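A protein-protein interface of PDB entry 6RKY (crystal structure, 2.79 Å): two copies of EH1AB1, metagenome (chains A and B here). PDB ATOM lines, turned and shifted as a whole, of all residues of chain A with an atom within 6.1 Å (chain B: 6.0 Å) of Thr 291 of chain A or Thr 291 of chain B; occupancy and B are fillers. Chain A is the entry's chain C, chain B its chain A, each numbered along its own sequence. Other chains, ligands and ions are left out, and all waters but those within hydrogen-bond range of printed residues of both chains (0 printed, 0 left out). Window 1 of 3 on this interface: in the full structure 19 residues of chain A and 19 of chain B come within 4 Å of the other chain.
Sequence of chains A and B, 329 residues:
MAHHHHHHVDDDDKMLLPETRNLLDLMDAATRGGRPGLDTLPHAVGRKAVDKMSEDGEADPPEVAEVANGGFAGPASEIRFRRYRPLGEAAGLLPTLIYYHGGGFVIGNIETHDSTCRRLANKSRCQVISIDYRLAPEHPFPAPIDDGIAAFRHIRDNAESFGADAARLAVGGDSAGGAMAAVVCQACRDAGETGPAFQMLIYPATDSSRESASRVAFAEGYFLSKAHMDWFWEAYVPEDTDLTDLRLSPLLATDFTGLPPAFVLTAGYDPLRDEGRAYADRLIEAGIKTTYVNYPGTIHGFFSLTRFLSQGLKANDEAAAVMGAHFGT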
ATOM      1  N   PHE A 198      -4.618  -9.079  14.782  1.00  0.00           N
ATOM      2  CA  PHE A 198      -3.707  -7.985  15.192  1.00  0.00           C
ATOM      3  C   PHE A 198      -3.198  -8.247  16.606  1.00  0.00           C
ATOM      4  O   PHE A 198      -3.979  -8.784  17.452  1.00  0.00           O
ATOM      5  CB  PHE A 198      -4.441  -6.659  15.106  1.00  0.00           C
ATOM      6  CG  PHE A 198      -3.542  -5.456  15.170  1.00  0.00           C
ATOM      7  CD1 PHE A 198      -3.104  -4.957  16.386  1.00  0.00           C
ATOM      8  CD2 PHE A 198      -3.166  -4.792  14.010  1.00  0.00           C
ATOM      9  CE1 PHE A 198      -2.291  -3.843  16.440  1.00  0.00           C
ATOM     10  CE2 PHE A 198      -2.366  -3.659  14.075  1.00  0.00           C
ATOM     11  CZ  PHE A 198      -1.938  -3.187  15.290  1.00  0.00           C
ATOM     12  N   ALA A 262       1.370  -6.343  13.781  1.00  0.00           N
ATOM     13  CA  ALA A 262       1.754  -6.026  15.164  1.00  0.00           C
ATOM     14  C   ALA A 262       2.019  -4.531  15.325  1.00  0.00           C
ATOM     15  O   ALA A 262       2.602  -3.928  14.425  1.00  0.00           O
ATOM     16  CB  ALA A 262       2.956  -6.823  15.514  1.00  0.00           C
ATOM     17  N   PHE A 263       1.575  -3.971  16.442  1.00  0.00           N
ATOM     18  CA  PHE A 263       2.069  -2.700  17.022  1.00  0.00           C
ATOM     19  C   PHE A 263       2.931  -3.037  18.247  1.00  0.00           C
ATOM     20  O   PHE A 263       2.516  -3.882  19.061  1.00  0.00           O
ATOM     21  CB  PHE A 263       0.878  -1.822  17.381  1.00  0.00           C
ATOM     22  CG  PHE A 263       1.226  -0.608  18.184  1.00  0.00           C
ATOM     23  CD1 PHE A 263       1.461   0.589  17.543  1.00  0.00           C
ATOM     24  CD2 PHE A 263       1.278  -0.654  19.565  1.00  0.00           C
ATOM     25  CE1 PHE A 263       1.777   1.730  18.260  1.00  0.00           C
ATOM     26  CE2 PHE A 263       1.599   0.479  20.292  1.00  0.00           C
ATOM     27  CZ  PHE A 263       1.865   1.666  19.636  1.00  0.00           C
ATOM     28  N   VAL A 264       4.126  -2.461  18.353  1.00  0.00           N
ATOM     29  CA  VAL A 264       5.070  -2.747  19.472  1.00  0.00           C
ATOM     30  C   VAL A 264       5.591  -1.413  20.016  1.00  0.00           C
ATOM     31  O   VAL A 264       6.064  -0.566  19.233  1.00  0.00           O
ATOM     32  CB  VAL A 264       6.210  -3.680  19.036  1.00  0.00           C
ATOM     33  CG1 VAL A 264       7.146  -4.003  20.181  1.00  0.00           C
ATOM     34  CG2 VAL A 264       5.680  -4.965  18.433  1.00  0.00           C
ATOM     35  N   LEU A 265       5.492  -1.246  21.333  1.00  0.00           N
ATOM     36  CA  LEU A 265       5.811   0.008  22.058  1.00  0.00           C
ATOM     37  C   LEU A 265       6.891  -0.297  23.086  1.00  0.00           C
ATOM     38  O   LEU A 265       6.817  -1.363  23.721  1.00  0.00           O
ATOM     39  CB  LEU A 265       4.545   0.551  22.729  1.00  0.00           C
ATOM     40  CG  LEU A 265       4.629   1.982  23.266  1.00  0.00           C
ATOM     41  CD1 LEU A 265       3.318   2.709  23.083  1.00  0.00           C
ATOM     42  CD2 LEU A 265       5.019   1.996  24.740  1.00  0.00           C
ATOM     43  N   ALA A 280      10.053  -6.813  17.451  1.00  0.00           N
ATOM     44  CA  ALA A 280       9.631  -5.929  16.334  1.00  0.00           C
ATOM     45  C   ALA A 280      10.502  -6.185  15.099  1.00  0.00           C
ATOM     46  O   ALA A 280       9.933  -6.358  14.013  1.00  0.00           O
ATOM     47  CB  ALA A 280       9.702  -4.486  16.761  1.00  0.00           C
ATOM     48  N   LYS A 289       3.313  -6.786   8.454  1.00  0.00           N
ATOM     49  CA  LYS A 289       2.989  -5.343   8.647  1.00  0.00           C
ATOM     50  C   LYS A 289       3.173  -5.050  10.140  1.00  0.00           C
ATOM     51  O   LYS A 289       2.673  -5.848  10.959  1.00  0.00           O
ATOM     52  CB  LYS A 289       1.596  -5.012   8.092  1.00  0.00           C
ATOM     53  CG  LYS A 289       0.781  -3.964   8.844  1.00  0.00           C
ATOM     54  CD  LYS A 289       1.146  -2.525   8.587  1.00  0.00           C
ATOM     55  CE  LYS A 289       0.305  -1.553   9.397  1.00  0.00           C
ATOM     56  NZ  LYS A 289      -1.156  -1.811   9.263  1.00  0.00           N
ATOM     57  N   THR A 290       3.916  -4.004  10.485  1.00  0.00           N
ATOM     58  CA  THR A 290       4.450  -3.819  11.857  1.00  0.00           C
ATOM     59  C   THR A 290       4.694  -2.333  12.093  1.00  0.00           C
ATOM     60  O   THR A 290       5.434  -1.726  11.332  1.00  0.00           O
ATOM     61  CB  THR A 290       5.773  -4.578  12.075  1.00  0.00           C
ATOM     62  OG1 THR A 290       5.705  -5.887  11.513  1.00  0.00           O
ATOM     63  CG2 THR A 290       6.167  -4.687  13.539  1.00  0.00           C
ATOM     64  N   THR A 291       4.101  -1.789  13.138  1.00  0.00           N
ATOM     65  CA  THR A 291       4.431  -0.449  13.677  1.00  0.00           C
ATOM     66  C   THR A 291       5.338  -0.639  14.892  1.00  0.00           C
ATOM     67  O   THR A 291       5.043  -1.516  15.717  1.00  0.00           O
ATOM     68  CB  THR A 291       3.155   0.308  14.017  1.00  0.00           C
ATOM     69  OG1 THR A 291       2.366   0.117  12.842  1.00  0.00           O
ATOM     70  CG2 THR A 291       3.414   1.761  14.357  1.00  0.00           C
ATOM     71  N   TYR A 292       6.433   0.111  14.942  1.00  0.00           N
ATOM     72  CA  TYR A 292       7.337   0.145  16.110  1.00  0.00           C
ATOM     73  C   TYR A 292       7.432   1.596  16.607  1.00  0.00           C
ATOM     74  O   TYR A 292       7.653   2.524  15.800  1.00  0.00           O
ATOM     75  CB  TYR A 292       8.700  -0.467  15.765  1.00  0.00           C
ATOM     76  CG  TYR A 292       9.650  -0.289  16.912  1.00  0.00           C
ATOM     77  CD1 TYR A 292       9.534  -1.084  18.042  1.00  0.00           C
ATOM     78  CD2 TYR A 292      10.525   0.791  16.950  1.00  0.00           C
ATOM     79  CE1 TYR A 292      10.296  -0.840  19.169  1.00  0.00           C
ATOM     80  CE2 TYR A 292      11.311   1.032  18.064  1.00  0.00           C
ATOM     81  CZ  TYR A 292      11.199   0.213  19.178  1.00  0.00           C
ATOM     82  OH  TYR A 292      11.965   0.436  20.282  1.00  0.00           O
ATOM     83  N   VAL A 293       7.227   1.807  17.905  1.00  0.00           N
ATOM     84  CA  VAL A 293       7.352   3.165  18.516  1.00  0.00           C
ATOM     85  C   VAL A 293       8.182   3.095  19.788  1.00  0.00           C
ATOM     86  O   VAL A 293       7.924   2.197  20.617  1.00  0.00           O
ATOM     87  CB  VAL A 293       5.994   3.833  18.795  1.00  0.00           C
ATOM     88  CG1 VAL A 293       5.107   2.965  19.638  1.00  0.00           C
ATOM     89  CG2 VAL A 293       6.181   5.217  19.408  1.00  0.00           C
ATOM     90  N   ASN A 294       9.120   4.031  19.933  1.00  0.00           N
ATOM     91  CA  ASN A 294       9.905   4.170  21.182  1.00  0.00           C
ATOM     92  C   ASN A 294       9.496   5.473  21.858  1.00  0.00           C
ATOM     93  O   ASN A 294       9.500   6.503  21.190  1.00  0.00           O
ATOM     94  CB  ASN A 294      11.420   4.093  20.951  1.00  0.00           C
ATOM     95  CG  ASN A 294      12.202   3.968  22.248  1.00  0.00           C
ATOM     96  OD1 ASN A 294      12.041   2.996  22.991  1.00  0.00           O
ATOM     97  ND2 ASN A 294      13.041   4.947  22.539  1.00  0.00           N
ATOM     98  N   TYR A 295       9.113   5.394  23.126  1.00  0.00           N
ATOM     99  CA  TYR A 295       8.868   6.561  24.008  1.00  0.00           C
ATOM    100  C   TYR A 295      10.104   6.731  24.869  1.00  0.00           C
ATOM    101  O   TYR A 295      10.206   6.136  25.929  1.00  0.00           O
ATOM    102  CB  TYR A 295       7.589   6.408  24.824  1.00  0.00           C
ATOM    103  CG  TYR A 295       6.358   6.789  24.054  1.00  0.00           C
ATOM    104  CD1 TYR A 295       5.796   5.934  23.118  1.00  0.00           C
ATOM    105  CD2 TYR A 295       5.745   8.006  24.268  1.00  0.00           C
ATOM    106  CE1 TYR A 295       4.661   6.285  22.402  1.00  0.00           C
ATOM    107  CE2 TYR A 295       4.604   8.371  23.570  1.00  0.00           C
ATOM    108  CZ  TYR A 295       4.064   7.516  22.626  1.00  0.00           C
ATOM    109  OH  TYR A 295       2.948   7.917  21.937  1.00  0.00           O
ATOM    110  N   GLU A 318      -1.891   6.739  20.822  1.00  0.00           N
ATOM    111  CA  GLU A 318      -1.146   6.230  19.645  1.00  0.00           C
ATOM    112  C   GLU A 318      -1.522   4.768  19.400  1.00  0.00           C
ATOM    113  O   GLU A 318      -1.836   4.453  18.246  1.00  0.00           O
ATOM    114  CB  GLU A 318       0.358   6.409  19.765  1.00  0.00           C
ATOM    115  CG  GLU A 318       0.996   6.472  18.388  1.00  0.00           C
ATOM    116  CD  GLU A 318       2.509   6.391  18.331  1.00  0.00           C
ATOM    117  OE1 GLU A 318       3.176   7.227  19.001  1.00  0.00           O
ATOM    118  OE2 GLU A 318       3.010   5.486  17.614  1.00  0.00           O
ATOM    119  N   VAL A 322      -3.628   3.589  15.950  1.00  0.00           N
ATOM    120  CA  VAL A 322      -3.037   2.578  15.019  1.00  0.00           C
ATOM    121  C   VAL A 322      -4.016   1.411  14.824  1.00  0.00           C
ATOM    122  O   VAL A 322      -4.160   0.969  13.672  1.00  0.00           O
ATOM    123  CB  VAL A 322      -1.676   2.074  15.506  1.00  0.00           C
ATOM    124  CG1 VAL A 322      -1.223   0.810  14.772  1.00  0.00           C
ATOM    125  CG2 VAL A 322      -0.633   3.162  15.379  1.00  0.00           C
ATOM    126  N   ALA B 262       9.368  11.914  15.075  1.00  0.00           N
ATOM    127  CA  ALA B 262       9.216  11.478  13.676  1.00  0.00           C
ATOM    128  C   ALA B 262       8.259  10.282  13.590  1.00  0.00           C
ATOM    129  O   ALA B 262       8.321   9.392  14.444  1.00  0.00           O
ATOM    130  CB  ALA B 262      10.571  11.144  13.103  1.00  0.00           C
ATOM    131  N   PHE B 263       7.426  10.283  12.560  1.00  0.00           N
ATOM    132  CA  PHE B 263       6.749   9.088  12.000  1.00  0.00           C
ATOM    133  C   PHE B 263       7.420   8.753  10.670  1.00  0.00           C
ATOM    134  O   PHE B 263       7.624   9.677   9.849  1.00  0.00           O
ATOM    135  CB  PHE B 263       5.253   9.360  11.837  1.00  0.00           C
ATOM    136  CG  PHE B 263       4.509   8.304  11.084  1.00  0.00           C
ATOM    137  CD1 PHE B 263       3.959   7.213  11.742  1.00  0.00           C
ATOM    138  CD2 PHE B 263       4.371   8.401   9.709  1.00  0.00           C
ATOM    139  CE1 PHE B 263       3.271   6.235  11.040  1.00  0.00           C
ATOM    140  CE2 PHE B 263       3.662   7.436   9.000  1.00  0.00           C
ATOM    141  CZ  PHE B 263       3.124   6.348   9.672  1.00  0.00           C
ATOM    142  N   VAL B 264       7.802   7.486  10.470  1.00  0.00           N
ATOM    143  CA  VAL B 264       8.428   7.039   9.196  1.00  0.00           C
ATOM    144  C   VAL B 264       7.667   5.807   8.677  1.00  0.00           C
ATOM    145  O   VAL B 264       7.459   4.857   9.437  1.00  0.00           O
ATOM    146  CB  VAL B 264       9.930   6.794   9.389  1.00  0.00           C
ATOM    147  CG1 VAL B 264      10.617   6.291   8.123  1.00  0.00           C
ATOM    148  CG2 VAL B 264      10.611   8.040   9.920  1.00  0.00           C
ATOM    149  N   LEU B 265       7.310   5.850   7.399  1.00  0.00           N
ATOM    150  CA  LEU B 265       6.600   4.774   6.678  1.00  0.00           C
ATOM    151  C   LEU B 265       7.459   4.270   5.508  1.00  0.00           C
ATOM    152  O   LEU B 265       8.115   5.098   4.836  1.00  0.00           O
ATOM    153  CB  LEU B 265       5.276   5.357   6.181  1.00  0.00           C
ATOM    154  CG  LEU B 265       4.238   4.346   5.702  1.00  0.00           C
ATOM    155  CD1 LEU B 265       2.841   4.779   6.133  1.00  0.00           C
ATOM    156  CD2 LEU B 265       4.338   4.202   4.185  1.00  0.00           C
ATOM    157  N   ALA B 280      15.096   6.114  10.233  1.00  0.00           N
ATOM    158  CA  ALA B 280      14.317   5.755  11.443  1.00  0.00           C
ATOM    159  C   ALA B 280      15.246   5.231  12.540  1.00  0.00           C
ATOM    160  O   ALA B 280      15.128   5.708  13.681  1.00  0.00           O
ATOM    161  CB  ALA B 280      13.265   4.742  11.103  1.00  0.00           C
ATOM    162  N   LYS B 289      11.763  10.442  20.053  1.00  0.00           N
ATOM    163  CA  LYS B 289      10.455   9.742  20.004  1.00  0.00           C
ATOM    164  C   LYS B 289      10.146   9.511  18.525  1.00  0.00           C
ATOM    165  O   LYS B 289      10.284  10.459  17.723  1.00  0.00           O
ATOM    166  CB  LYS B 289       9.391  10.554  20.761  1.00  0.00           C
ATOM    167  CG  LYS B 289       7.969  10.507  20.203  1.00  0.00           C
ATOM    168  CD  LYS B 289       7.174   9.269  20.530  1.00  0.00           C
ATOM    169  CE  LYS B 289       5.965   9.077  19.629  1.00  0.00           C
ATOM    170  NZ  LYS B 289       5.188  10.331  19.411  1.00  0.00           N
ATOM    171  N   THR B 290       9.802   8.284  18.154  1.00  0.00           N
ATOM    172  CA  THR B 290       9.833   7.828  16.743  1.00  0.00           C
ATOM    173  C   THR B 290       8.867   6.665  16.590  1.00  0.00           C
ATOM    174  O   THR B 290       9.021   5.697  17.329  1.00  0.00           O
ATOM    175  CB  THR B 290      11.245   7.374  16.302  1.00  0.00           C
ATOM    176  OG1 THR B 290      12.247   8.299  16.731  1.00  0.00           O
ATOM    177  CG2 THR B 290      11.392   7.207  14.803  1.00  0.00           C
ATOM    178  N   THR B 291       7.938   6.765  15.647  1.00  0.00           N
ATOM    179  CA  THR B 291       7.131   5.617  15.173  1.00  0.00           C
ATOM    180  C   THR B 291       7.708   5.159  13.842  1.00  0.00           C
ATOM    181  O   THR B 291       8.035   6.028  13.013  1.00  0.00           O
ATOM    182  CB  THR B 291       5.660   6.029  15.089  1.00  0.00           C
ATOM    183  OG1 THR B 291       5.402   6.593  16.376  1.00  0.00           O
ATOM    184  CG2 THR B 291       4.729   4.876  14.778  1.00  0.00           C
ATOM    185  N   TYR B 292       7.856   3.861  13.645  1.00  0.00           N
ATOM    186  CA  TYR B 292       8.334   3.268  12.369  1.00  0.00           C
ATOM    187  C   TYR B 292       7.317   2.200  11.936  1.00  0.00           C
ATOM    188  O   TYR B 292       6.974   1.311  12.769  1.00  0.00           O
ATOM    189  CB  TYR B 292       9.779   2.725  12.464  1.00  0.00           C
ATOM    190  CG  TYR B 292      10.145   2.009  11.198  1.00  0.00           C
ATOM    191  CD1 TYR B 292      10.445   2.707  10.041  1.00  0.00           C
ATOM    192  CD2 TYR B 292      10.000   0.637  11.098  1.00  0.00           C
ATOM    193  CE1 TYR B 292      10.653   2.061   8.832  1.00  0.00           C
ATOM    194  CE2 TYR B 292      10.206  -0.030   9.897  1.00  0.00           C
ATOM    195  CZ  TYR B 292      10.528   0.691   8.764  1.00  0.00           C
ATOM    196  OH  TYR B 292      10.733   0.023   7.603  1.00  0.00           O
ATOM    197  N   VAL B 293       6.849   2.261  10.686  1.00  0.00           N
ATOM    198  CA  VAL B 293       5.891   1.256  10.147  1.00  0.00           C
ATOM    199  C   VAL B 293       6.333   0.794   8.764  1.00  0.00           C
ATOM    200  O   VAL B 293       6.672   1.656   7.924  1.00  0.00           O
ATOM    201  CB  VAL B 293       4.433   1.766  10.112  1.00  0.00           C
ATOM    202  CG1 VAL B 293       4.293   3.044   9.303  1.00  0.00           C
ATOM    203  CG2 VAL B 293       3.518   0.669   9.555  1.00  0.00           C
ATOM    204  N   ASN B 294       6.306  -0.512   8.530  1.00  0.00           N
ATOM    205  CA  ASN B 294       6.604  -1.092   7.193  1.00  0.00           C
ATOM    206  C   ASN B 294       5.310  -1.713   6.673  1.00  0.00           C
ATOM    207  O   ASN B 294       4.669  -2.509   7.425  1.00  0.00           O
ATOM    208  CB  ASN B 294       7.728  -2.136   7.208  1.00  0.00           C
ATOM    209  CG  ASN B 294       8.174  -2.542   5.817  1.00  0.00           C
ATOM    210  OD1 ASN B 294       8.657  -1.715   5.034  1.00  0.00           O
ATOM    211  ND2 ASN B 294       8.027  -3.821   5.499  1.00  0.00           N
ATOM    212  N   GLU B 318      -3.218   5.609   9.370  1.00  0.00           N
ATOM    213  CA  GLU B 318      -2.167   5.377  10.392  1.00  0.00           C
ATOM    214  C   GLU B 318      -1.336   6.652  10.577  1.00  0.00           C
ATOM    215  O   GLU B 318      -1.145   7.039  11.718  1.00  0.00           O
ATOM    216  CB  GLU B 318      -1.289   4.172  10.084  1.00  0.00           C
ATOM    217  CG  GLU B 318      -0.659   3.637  11.357  1.00  0.00           C
ATOM    218  CD  GLU B 318       0.389   2.551  11.200  1.00  0.00           C
ATOM    219  OE1 GLU B 318       0.142   1.516  10.472  1.00  0.00           O
ATOM    220  OE2 GLU B 318       1.426   2.725  11.832  1.00  0.00           O
ATOM    221  N   VAL B 322      -1.441   8.768  14.186  1.00  0.00           N
ATOM    222  CA  VAL B 322      -0.178   8.996  14.950  1.00  0.00           C
ATOM    223  C   VAL B 322       0.027  10.493  15.200  1.00  0.00           C
ATOM    224  O   VAL B 322       0.420  10.844  16.320  1.00  0.00           O
ATOM    225  CB  VAL B 322       1.040   8.390  14.234  1.00  0.00           C
ATOM    226  CG1 VAL B 322       2.364   8.910  14.787  1.00  0.00           C
ATOM    227  CG2 VAL B 322       0.995   6.870  14.296  1.00  0.00           C
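NZ of Lys 289 of chain B is in salt-bridge range of OE1 of Glu 318 of chain A (3.7 Å).
The backbone NH (N) of Asn 294 of chain A lies within hydrogen-bond range of the backbone carbonyl oxygen (O) of Thr 290 of chain B (3.1 Å).
The side-chain hydroxyl (OG1) of Thr 291 of chain B is in hydrogen-bond range of the side-chain carboxylate (OE2) of Glu 318 of chain A (2.9 Å).
The backbone carbonyl oxygen (O) of Tyr 292 of chain B is in hydrogen-bond range of the backbone NH (N) of Tyr 292 of chain A (2.5 Å).
The backbone carbonyl oxygen of Thr 290 of chain A sits at hydrogen-bond distance from the backbone NH of Asn 294 of chain B.
NZ of Lys 289 of chain A lies within salt-bridge range of OE1 of Glu 318 of chain B (3.8 Å).
The side-chain carboxylate (OE2) of Glu 318 of chain B lies within hydrogen-bond range of the side-chain hydroxyl (OG1) of Thr 291 of chain A (3.0 Å).
The backbone NH of Ala 262 of chain B is in hydrogen-bond range of the backbone carbonyl oxygen of Lys 289 of chain B (3.2 Å).
The backbone NH (N) of Thr 291 of chain B is in hydrogen-bond range of the backbone carbonyl oxygen (O) of Ala 262 of chain B, at 2.9 Å.
The backbone NH (N) of Val 293 of chain B lies within hydrogen-bond range of the backbone carbonyl oxygen (O) of Val 264 of chain B, 2.9 Å away.
The backbone carbonyl oxygen (O) of Lys 289 of chain A lies within hydrogen-bond range of the backbone NH (N) of Ala 262 of chain A (3.1 Å).
N of Val 264 of chain A lies within hydrogen-bond range of O of Thr 291 of chain A (2.9 Å).
O of Val 264 of chain A lies within hydrogen-bond range of N of Val 293 of chain A, 3.0 Å away.
Among the printed residues, merely in contact across the chains: Lys 289 of chain A with Val 293 of chain B, Lys 289 of chain A with Asn 294 of chain B, Thr 290 of chain A with Tyr 292 of chain B, Thr 290 of chain A with Val 293 of chain B, Thr 291 of chain A with Thr 291 of chain B, Thr 291 of chain A with Tyr 292 of chain B, Thr 291 of chain A with Val 293 of chain B, Tyr 292 of chain A with Thr 290 of chain B, Tyr 292 of chain A with Thr 291 of chain B, Val 293 of chain A with Lys 289 of chain B, Val 293 of chain A with Thr 290 of chain B, Val 293 of chain A with Thr 291 of chain B, Asn 294 of chain A with Lys 289 of chain B and Tyr 295 of chain A with Lys 289 of chain B.
Of chain B, only Thr 291, Tyr 292, Val 293 and Glu 318 come within 4 Å of Thr 291 of chain A.
Thr 291 of chain B touches just these residues of chain A: Thr 291 (3.4 Å), Tyr 292 (3.2 Å), Val 293 (3.4 Å) and Glu 318 (2.9 Å).
Of the printed residues of chain B, Val 293 of chain A touches Lys 289 (3.9 Å), Thr 290 (3.3 Å) and Thr 291 (3.4 Å).
Printed residues of chain A within 4 Å of Val 293 of chain B: Lys 289, Thr 290 and Thr 291.
Of the printed residues of chain B, Tyr 295 of chain A touches Lys 289 (3.9 Å).
The nearest printed residue of chain B that does not touch Tyr 292 of chain A is Val 293 of chain B (4.8 Å).
Of the 13 printed residues of chain B, 7 touch a printed residue of chain A.
Hydrophobic or aromatic side chains of chain B within 4 Å of the printed part of chain A: Tyr 292 and Val 293.
Of the 15 printed residues of chain A, 8 touch a printed residue of chain B.
Among the printed residues, 21 pairs touch across the chains.
Among the printed residues, Asp or Glu carboxylates within 4 Å of a Lys or Arg side-chain nitrogen of the other chain: Lys 289 of chain A with Glu 318 of chain B and Glu 318 of chain A with Lys 289 of chain B.
Lys 289 of chain A touches Val 293 of chain B, and with the chains exchanged Val 293 of chain A touches Lys 289 of chain B.
Lys 289 of chain A touches Asn 294 of chain B, and with the chains exchanged Asn 294 of chain A touches Lys 289 of chain B.
Thr 290 of chain A touches Tyr 292 of chain B, and with the chains exchanged Tyr 292 of chain A touches Thr 290 of chain B.
Thr 291 of chain A touches its own counterpart, Thr 291 of chain B.
Of the 21 pairs that touch across the chains among the printed residues, 20 have their exchanged pair printed and touching as well.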
